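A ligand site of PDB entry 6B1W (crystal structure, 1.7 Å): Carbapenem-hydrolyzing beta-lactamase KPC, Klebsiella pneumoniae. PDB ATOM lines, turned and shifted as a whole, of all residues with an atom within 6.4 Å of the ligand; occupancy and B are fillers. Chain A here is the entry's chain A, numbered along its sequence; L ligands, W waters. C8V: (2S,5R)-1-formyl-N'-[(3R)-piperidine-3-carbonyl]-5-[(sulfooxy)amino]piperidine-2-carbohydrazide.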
ATOM      1  N   LEU A  46      24.411  14.882   2.582  1.00  0.00           N
ATOM      2  CA  LEU A  46      24.589  13.562   3.127  1.00  0.00           C
ATOM      3  C   LEU A  46      23.537  13.202   4.172  1.00  0.00           C
ATOM      4  O   LEU A  46      23.068  12.049   4.213  1.00  0.00           O
ATOM      5  CB  LEU A  46      25.993  13.410   3.703  1.00  0.00           C
ATOM      6  CG  LEU A  46      27.080  13.419   2.622  1.00  0.00           C
ATOM      7  CD1 LEU A  46      28.431  13.803   3.199  1.00  0.00           C
ATOM      8  CD2 LEU A  46      27.176  12.085   1.909  1.00  0.00           C
ATOM      9  N   CYS A  47      23.161  14.151   5.032  1.00  0.00           N
ATOM     10  CA  CYS A  47      22.323  13.812   6.185  1.00  0.00           C
ATOM     11  C   CYS A  47      23.017  12.686   6.993  1.00  0.00           C
ATOM     12  O   CYS A  47      24.242  12.660   7.036  1.00  0.00           O
ATOM     13  CB  CYS A  47      20.883  13.476   5.747  1.00  0.00           C
ATOM     14  SG  CYS A  47      20.187  14.602   4.522  1.00  0.00           S
ATOM     15  N   SER A  48      22.278  11.718   7.536  1.00  0.00           N
ATOM     16  CA  SER A  48      22.872  10.629   8.269  1.00  0.00           C
ATOM     17  C   SER A  48      23.699   9.647   7.444  1.00  0.00           C
ATOM     18  O   SER A  48      24.393   8.830   8.030  1.00  0.00           O
ATOM     19  CB  SER A  48      21.818   9.757   8.951  1.00  0.00           C
ATOM     20  OG  SER A  48      21.143  10.399   9.994  1.00  0.00           O
ATOM     21  N   SER A  49      23.646   9.721   6.115  1.00  0.00           N
ATOM     22  CA  SER A  49      24.310   8.736   5.282  1.00  0.00           C
ATOM     23  C   SER A  49      25.849   8.793   5.408  1.00  0.00           C
ATOM     24  O   SER A  49      26.521   7.844   5.089  1.00  0.00           O
ATOM     25  CB  SER A  49      23.859   8.865   3.828  1.00  0.00           C
ATOM     26  OG  SER A  49      24.483   9.962   3.184  1.00  0.00           O
ATOM     27  N   LYS A  51      27.375   8.328   8.021  1.00  0.00           N
ATOM     28  CA  LYS A  51      27.703   7.391   9.095  1.00  0.00           C
ATOM     29  C   LYS A  51      28.244   6.059   8.595  1.00  0.00           C
ATOM     30  O   LYS A  51      28.995   5.403   9.307  1.00  0.00           O
ATOM     31  CB  LYS A  51      26.467   7.177   9.983  1.00  0.00           C
ATOM     32  CG  LYS A  51      26.150   8.410  10.798  1.00  0.00           C
ATOM     33  CD  LYS A  51      24.774   8.359  11.432  1.00  0.00           C
ATOM     34  CE  LYS A  51      24.536   9.702  12.121  1.00  0.00           C
ATOM     35  NZ  LYS A  51      23.115   9.973  12.420  1.00  0.00           N
ATOM     36  N   PRO A  82      19.358  14.677  20.271  1.00  0.00           N
ATOM     37  CA  PRO A  82      18.205  13.870  19.865  1.00  0.00           C
ATOM     38  C   PRO A  82      18.552  12.941  18.685  1.00  0.00           C
ATOM     39  O   PRO A  82      19.527  13.196  17.958  1.00  0.00           O
ATOM     40  CB  PRO A  82      17.155  14.894  19.435  1.00  0.00           C
ATOM     41  CG  PRO A  82      17.712  16.227  19.741  1.00  0.00           C
ATOM     42  CD  PRO A  82      19.116  16.121  20.211  1.00  0.00           C
ATOM     43  N   TRP A  83      17.762  11.870  18.547  1.00  0.00           N
ATOM     44  CA  TRP A  83      17.989  10.740  17.626  1.00  0.00           C
ATOM     45  C   TRP A  83      19.300  10.008  17.923  1.00  0.00           C
ATOM     46  O   TRP A  83      20.133   9.769  17.050  1.00  0.00           O
ATOM     47  CB  TRP A  83      17.898  11.125  16.132  1.00  0.00           C
ATOM     48  CG  TRP A  83      16.566  11.641  15.666  1.00  0.00           C
ATOM     49  CD1 TRP A  83      15.521  10.909  15.235  1.00  0.00           C
ATOM     50  CD2 TRP A  83      16.146  13.026  15.611  1.00  0.00           C
ATOM     51  NE1 TRP A  83      14.473  11.739  14.879  1.00  0.00           N
ATOM     52  CE2 TRP A  83      14.824  13.033  15.118  1.00  0.00           C
ATOM     53  CE3 TRP A  83      16.756  14.241  15.940  1.00  0.00           C
ATOM     54  CZ2 TRP A  83      14.111  14.216  14.903  1.00  0.00           C
ATOM     55  CZ3 TRP A  83      16.030  15.422  15.707  1.00  0.00           C
ATOM     56  CH2 TRP A  83      14.712  15.388  15.210  1.00  0.00           C
ATOM     57  N   SER A  84      19.437   9.624  19.165  1.00  0.00           N
ATOM     58  CA  SER A  84      20.577   8.885  19.650  1.00  0.00           C
ATOM     59  C   SER A  84      20.068   7.776  20.601  1.00  0.00           C
ATOM     60  O   SER A  84      20.459   7.727  21.784  1.00  0.00           O
ATOM     61  CB  SER A  84      21.498   9.852  20.405  1.00  0.00           C
ATOM     62  OG  SER A  84      22.035  10.856  19.561  1.00  0.00           O
ATOM     63  N   PRO A  85      19.206   6.883  20.090  1.00  0.00           N
ATOM     64  CA  PRO A  85      18.471   5.938  20.945  1.00  0.00           C
ATOM     65  C   PRO A  85      19.406   4.935  21.664  1.00  0.00           C
ATOM     66  O   PRO A  85      19.144   4.592  22.845  1.00  0.00           O
ATOM     67  CB  PRO A  85      17.549   5.234  19.958  1.00  0.00           C
ATOM     68  CG  PRO A  85      18.231   5.357  18.647  1.00  0.00           C
ATOM     69  CD  PRO A  85      18.839   6.727  18.682  1.00  0.00           C
ATOM     70  N   TYR A 107      21.231   2.052  13.534  1.00  0.00           N
ATOM     71  CA  TYR A 107      20.195   2.879  14.139  1.00  0.00           C
ATOM     72  C   TYR A 107      20.353   4.374  13.814  1.00  0.00           C
ATOM     73  O   TYR A 107      19.562   5.168  14.270  1.00  0.00           O
ATOM     74  CB  TYR A 107      20.177   2.635  15.665  1.00  0.00           C
ATOM     75  CG  TYR A 107      19.644   1.232  15.929  1.00  0.00           C
ATOM     76  CD1 TYR A 107      18.265   0.995  15.966  1.00  0.00           C
ATOM     77  CD2 TYR A 107      20.515   0.163  16.015  1.00  0.00           C
ATOM     78  CE1 TYR A 107      17.758  -0.281  16.146  1.00  0.00           C
ATOM     79  CE2 TYR A 107      20.010  -1.129  16.191  1.00  0.00           C
ATOM     80  CZ  TYR A 107      18.655  -1.338  16.263  1.00  0.00           C
ATOM     81  OH  TYR A 107      18.179  -2.613  16.376  1.00  0.00           O
ATOM     82  N   SER A 108      21.363   4.738  13.027  1.00  0.00           N
ATOM     83  CA  SER A 108      21.610   6.122  12.681  1.00  0.00           C
ATOM     84  C   SER A 108      21.799   7.018  13.887  1.00  0.00           C
ATOM     85  O   SER A 108      21.411   8.195  13.885  1.00  0.00           O
ATOM     86  CB  SER A 108      20.459   6.602  11.786  1.00  0.00           C
ATOM     87  OG  SER A 108      20.937   7.515  10.843  1.00  0.00           O
ATOM     88  N   ASP A 109      22.444   6.489  14.927  1.00  0.00           N
ATOM     89  CA  ASP A 109      22.523   7.172  16.209  1.00  0.00           C
ATOM     90  C   ASP A 109      23.419   8.396  16.025  1.00  0.00           C
ATOM     91  O   ASP A 109      24.555   8.269  15.592  1.00  0.00           O
ATOM     92  CB  ASP A 109      23.116   6.185  17.211  1.00  0.00           C
ATOM     93  CG  ASP A 109      23.097   6.640  18.632  1.00  0.00           C
ATOM     94  OD1 ASP A 109      22.460   5.930  19.475  1.00  0.00           O
ATOM     95  OD2 ASP A 109      23.788   7.617  18.954  1.00  0.00           O
ATOM     96  N   ASN A 110      22.881   9.571  16.351  1.00  0.00           N
ATOM     97  CA  ASN A 110      23.629  10.847  16.182  1.00  0.00           C
ATOM     98  C   ASN A 110      24.832  11.043  17.120  1.00  0.00           C
ATOM     99  O   ASN A 110      25.940  11.347  16.664  1.00  0.00           O
ATOM    100  CB  ASN A 110      22.664  12.044  16.307  1.00  0.00           C
ATOM    101  CG  ASN A 110      21.845  12.294  15.029  1.00  0.00           C
ATOM    102  OD1 ASN A 110      22.259  11.925  13.954  1.00  0.00           O
ATOM    103  ND2 ASN A 110      20.691  12.956  15.158  1.00  0.00           N
ATOM    104  N   GLU A 144      26.782  16.406  13.987  1.00  0.00           N
ATOM    105  CA  GLU A 144      25.354  16.300  14.319  1.00  0.00           C
ATOM    106  C   GLU A 144      24.965  17.356  15.372  1.00  0.00           C
ATOM    107  O   GLU A 144      25.680  17.494  16.375  1.00  0.00           O
ATOM    108  CB  GLU A 144      25.025  14.883  14.812  1.00  0.00           C
ATOM    109  CG  GLU A 144      25.155  13.797  13.742  1.00  0.00           C
ATOM    110  CD  GLU A 144      24.076  13.901  12.692  1.00  0.00           C
ATOM    111  OE1 GLU A 144      23.239  14.823  12.807  1.00  0.00           O
ATOM    112  OE2 GLU A 144      24.021  13.023  11.780  1.00  0.00           O
ATOM    113  N   LEU A 145      23.879  18.111  15.219  1.00  0.00           N
ATOM    114  CA  LEU A 145      22.834  18.014  14.199  1.00  0.00           C
ATOM    115  C   LEU A 145      22.954  19.043  13.074  1.00  0.00           C
ATOM    116  O   LEU A 145      22.177  19.011  12.100  1.00  0.00           O
ATOM    117  CB  LEU A 145      21.480  18.287  14.877  1.00  0.00           C
ATOM    118  CG  LEU A 145      21.025  17.293  15.944  1.00  0.00           C
ATOM    119  CD1 LEU A 145      20.113  17.972  16.958  1.00  0.00           C
ATOM    120  CD2 LEU A 145      20.278  16.177  15.277  1.00  0.00           C
ATOM    121  N   GLU A 146      23.933  19.950  13.163  1.00  0.00           N
ATOM    122  CA  GLU A 146      23.969  21.080  12.246  1.00  0.00           C
ATOM    123  C   GLU A 146      24.180  20.646  10.787  1.00  0.00           C
ATOM    124  O   GLU A 146      23.705  21.339   9.867  1.00  0.00           O
ATOM    125  CB  GLU A 146      25.054  22.073  12.638  1.00  0.00           C
ATOM    126  CG  GLU A 146      24.766  22.704  13.967  1.00  0.00           C
ATOM    127  CD  GLU A 146      25.302  21.968  15.191  1.00  0.00           C
ATOM    128  OE1 GLU A 146      25.873  20.833  15.149  1.00  0.00           O
ATOM    129  OE2 GLU A 146      25.119  22.590  16.265  1.00  0.00           O
ATOM    130  N   ASN A 148      22.743  18.590   9.080  1.00  0.00           N
ATOM    131  CA  ASN A 148      21.482  18.289   8.390  1.00  0.00           C
ATOM    132  C   ASN A 148      20.741  19.491   7.803  1.00  0.00           C
ATOM    133  O   ASN A 148      19.660  19.296   7.304  1.00  0.00           O
ATOM    134  CB  ASN A 148      20.522  17.609   9.383  1.00  0.00           C
ATOM    135  CG  ASN A 148      21.038  16.282   9.858  1.00  0.00           C
ATOM    136  OD1 ASN A 148      21.168  15.352   9.061  1.00  0.00           O
ATOM    137  ND2 ASN A 148      21.393  16.196  11.144  1.00  0.00           N
ATOM    138  N   SER A 149      21.300  20.706   7.869  1.00  0.00           N
ATOM    139  CA  SER A 149      20.522  21.894   7.500  1.00  0.00           C
ATOM    140  C   SER A 149      20.029  21.864   6.072  1.00  0.00           C
ATOM    141  O   SER A 149      18.953  22.374   5.793  1.00  0.00           O
ATOM    142  CB  SER A 149      21.304  23.195   7.778  1.00  0.00           C
ATOM    143  OG  SER A 149      22.610  23.115   7.259  1.00  0.00           O
ATOM    144  N   THR A 194      17.068   0.794   9.511  1.00  0.00           N
ATOM    145  CA  THR A 194      16.326   1.997   9.109  1.00  0.00           C
ATOM    146  C   THR A 194      15.943   2.104   7.637  1.00  0.00           C
ATOM    147  O   THR A 194      15.308   3.096   7.228  1.00  0.00           O
ATOM    148  CB  THR A 194      17.117   3.255   9.446  1.00  0.00           C
ATOM    149  OG1 THR A 194      18.273   3.320   8.616  1.00  0.00           O
ATOM    150  CG2 THR A 194      17.500   3.226  10.905  1.00  0.00           C
ATOM    151  N   LYS A 212      22.812   2.238   4.025  1.00  0.00           N
ATOM    152  CA  LYS A 212      22.744   3.320   5.018  1.00  0.00           C
ATOM    153  C   LYS A 212      21.879   4.462   4.479  1.00  0.00           C
ATOM    154  O   LYS A 212      22.095   4.943   3.384  1.00  0.00           O
ATOM    155  CB  LYS A 212      24.137   3.855   5.408  1.00  0.00           C
ATOM    156  CG  LYS A 212      24.103   5.030   6.389  1.00  0.00           C
ATOM    157  CD  LYS A 212      23.766   4.550   7.778  1.00  0.00           C
ATOM    158  CE  LYS A 212      23.272   5.638   8.732  1.00  0.00           C
ATOM    159  NZ  LYS A 212      21.822   5.937   8.671  1.00  0.00           N
ATOM    160  N   THR A 213      20.963   4.910   5.319  1.00  0.00           N
ATOM    161  CA  THR A 213      19.978   5.952   4.990  1.00  0.00           C
ATOM    162  C   THR A 213      20.408   7.319   5.503  1.00  0.00           C
ATOM    163  O   THR A 213      21.278   7.409   6.330  1.00  0.00           O
ATOM    164  CB  THR A 213      18.638   5.590   5.657  1.00  0.00           C
ATOM    165  OG1 THR A 213      18.811   5.485   7.067  1.00  0.00           O
ATOM    166  CG2 THR A 213      18.120   4.263   5.121  1.00  0.00           C
ATOM    167  N   GLY A 214      19.735   8.367   5.022  1.00  0.00           N
ATOM    168  CA  GLY A 214      19.824   9.709   5.564  1.00  0.00           C
ATOM    169  C   GLY A 214      18.504  10.399   5.396  1.00  0.00           C
ATOM    170  O   GLY A 214      17.838  10.193   4.397  1.00  0.00           O
ATOM    171  N   THR A 215      18.103  11.173   6.392  1.00  0.00           N
ATOM    172  CA  THR A 215      16.884  11.950   6.313  1.00  0.00           C
ATOM    173  C   THR A 215      17.109  13.285   7.001  1.00  0.00           C
ATOM    174  O   THR A 215      17.047  13.341   8.228  1.00  0.00           O
ATOM    175  CB  THR A 215      15.735  11.222   7.027  1.00  0.00           C
ATOM    176  OG1 THR A 215      15.684   9.870   6.601  1.00  0.00           O
ATOM    177  CG2 THR A 215      14.395  11.835   6.691  1.00  0.00           C
ATOM    178  N   CYS A 216      17.350  14.354   6.252  1.00  0.00           N
ATOM    179  CA  CYS A 216      17.668  15.655   6.871  1.00  0.00           C
ATOM    180  C   CYS A 216      16.486  16.332   7.588  1.00  0.00           C
ATOM    181  O   CYS A 216      16.706  17.228   8.426  1.00  0.00           O
ATOM    182  CB  CYS A 216      18.250  16.639   5.862  1.00  0.00           C
ATOM    183  SG  CYS A 216      20.012  16.407   5.486  1.00  0.00           S
ATOM    184  N   GLY A 217      15.275  15.947   7.215  1.00  0.00           N
ATOM    185  CA  GLY A 217      14.029  16.458   7.835  1.00  0.00           C
ATOM    186  C   GLY A 217      13.534  17.767   7.251  1.00  0.00           C
ATOM    187  O   GLY A 217      12.570  18.344   7.768  1.00  0.00           O
ATOM    188  N   VAL A 218      14.189  18.251   6.190  1.00  0.00           N
ATOM    189  CA  VAL A 218      13.889  19.549   5.559  1.00  0.00           C
ATOM    190  C   VAL A 218      14.276  19.501   4.081  1.00  0.00           C
ATOM    191  O   VAL A 218      15.047  18.662   3.666  1.00  0.00           O
ATOM    192  CB  VAL A 218      14.727  20.701   6.183  1.00  0.00           C
ATOM    193  CG1 VAL A 218      14.140  21.110   7.526  1.00  0.00           C
ATOM    194  CG2 VAL A 218      16.218  20.322   6.300  1.00  0.00           C
HETATM  195  NAR C8V L   1      18.123   8.850  13.274  1.00  0.00           N
HETATM  196  CAV C8V L   1      18.176   9.941  12.538  1.00  0.00           C
HETATM  197  CAK C8V L   1      16.917  10.416  12.129  1.00  0.00           C
HETATM  198  CB  C8V L   1      17.005  11.304  10.920  1.00  0.00           C
HETATM  199  CAN C8V L   1      19.455  10.463  12.206  1.00  0.00           C
HETATM  200  N   C8V L   1      19.306  11.311  10.980  1.00  0.00           N
HETATM  201  CAG C8V L   1      20.077  11.153   9.889  1.00  0.00           C
HETATM  202  OAA C8V L   1      19.792  11.464   8.763  1.00  0.00           O
HETATM  203  CA  C8V L   1      18.201  12.152  11.061  1.00  0.00           C
HETATM  204  C   C8V L   1      18.269  13.327  11.833  1.00  0.00           C
HETATM  205  O   C8V L   1      19.300  13.600  12.472  1.00  0.00           O
HETATM  206  NAQ C8V L   1      17.111  13.999  12.025  1.00  0.00           N
HETATM  207  NAP C8V L   1      17.191  15.175  12.682  1.00  0.00           N
HETATM  208  CAT C8V L   1      17.530  16.292  12.005  1.00  0.00           C
HETATM  209  OAB C8V L   1      18.061  16.259  10.916  1.00  0.00           O
HETATM  210  CAW C8V L   1      17.257  17.621  12.728  1.00  0.00           C
HETATM  211  CAJ C8V L   1      15.770  17.952  12.780  1.00  0.00           C
HETATM  212  CAH C8V L   1      15.209  18.093  11.384  1.00  0.00           C
HETATM  213  CAI C8V L   1      15.968  19.261  10.756  1.00  0.00           C
HETATM  214  NAO C8V L   1      17.416  19.033  10.693  1.00  0.00           N
HETATM  215  CAM C8V L   1      17.955  18.785  12.033  1.00  0.00           C
HETATM  216  O   HOH W   1      15.133  14.212  10.200  1.00  0.00           O
HETATM  217  O   HOH W   2      19.519  20.961  10.591  1.00  0.00           O
HETATM  218  O   HOH W   3      21.774  13.189  10.631  1.00  0.00           O
HETATM  219  O   HOH W   4      16.087   6.539  12.296  1.00  0.00           O
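Cys 47 touches the ligand. NZ of Lys 51 touches CAN of the ligand, at 3.7 Å. CZ3 of Trp 83 touches NAP of the ligand, 3.2 Å away. Leu 145 touches the ligand. Gly 214 touches the ligand (CA to OAA, 3.6 Å).
The side-chain hydroxyl (OG) of Ser 48 sits at hydrogen-bond distance from the side-chain hydroxyl (OG) of Ser 108 (3.0 Å). The side-chain sulfur (SG) of Cys 216 forms a disulfide with the side-chain sulfur (SG) of Cys 47, 2.1 Å away. The side-chain amide oxygen of Asn 110 sits close to the side-chain carboxylate of Glu 144 (3.0 Å). The side-chain amide nitrogen of Asn 110 lies within hydrogen-bond range of the backbone carbonyl oxygen of Pro 82 (3.0 Å). ND2 of Asn 148 is in hydrogen-bond range of O of Leu 145, at 3.1 Å. The side-chain amide nitrogen (ND2) of Asn 148 is in hydrogen-bond range of the side-chain carboxylate (OE1) of Glu 144, 2.8 Å away. The side-chain amino group of Lys 212 lies within hydrogen-bond range of the side-chain hydroxyl of Ser 108 (2.8 Å). The side-chain carboxylate (OE2) of Glu 144 lies within salt-bridge range of the side-chain amino group (NZ) of Lys 51 (3.2 Å).
Water W1 lies within hydrogen-bond range of NAQ of the ligand, O of Thr 215 and N of Gly 217. Water W2 bridges NAO of the ligand (2.9 Å) and N of Ser 149 (3.3 Å).
The backbone NH of Ser 48 lies close to an oxygen (OAA) of the ligand, 2.8 Å away. OG of Ser 48 is covalently linked to CAG of the ligand (1.3 Å). The backbone NH (N) of Thr 215 is in hydrogen-bond range of an oxygen (OAA) of the ligand, at 2.9 Å. The backbone carbonyl oxygen (O) of Cys 216 sits at hydrogen-bond distance from a nitrogen (NAO) of the ligand (3.0 Å). O of the ligand lies within hydrogen-bond range of ND2 of Asn 110. ND2 of Asn 148 sits close to OAB of the ligand, at 3.3 Å. The backbone carbonyl oxygen of Ser 108 lies within hydrogen-bond range of a nitrogen (NAR) of the ligand (3.4 Å).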
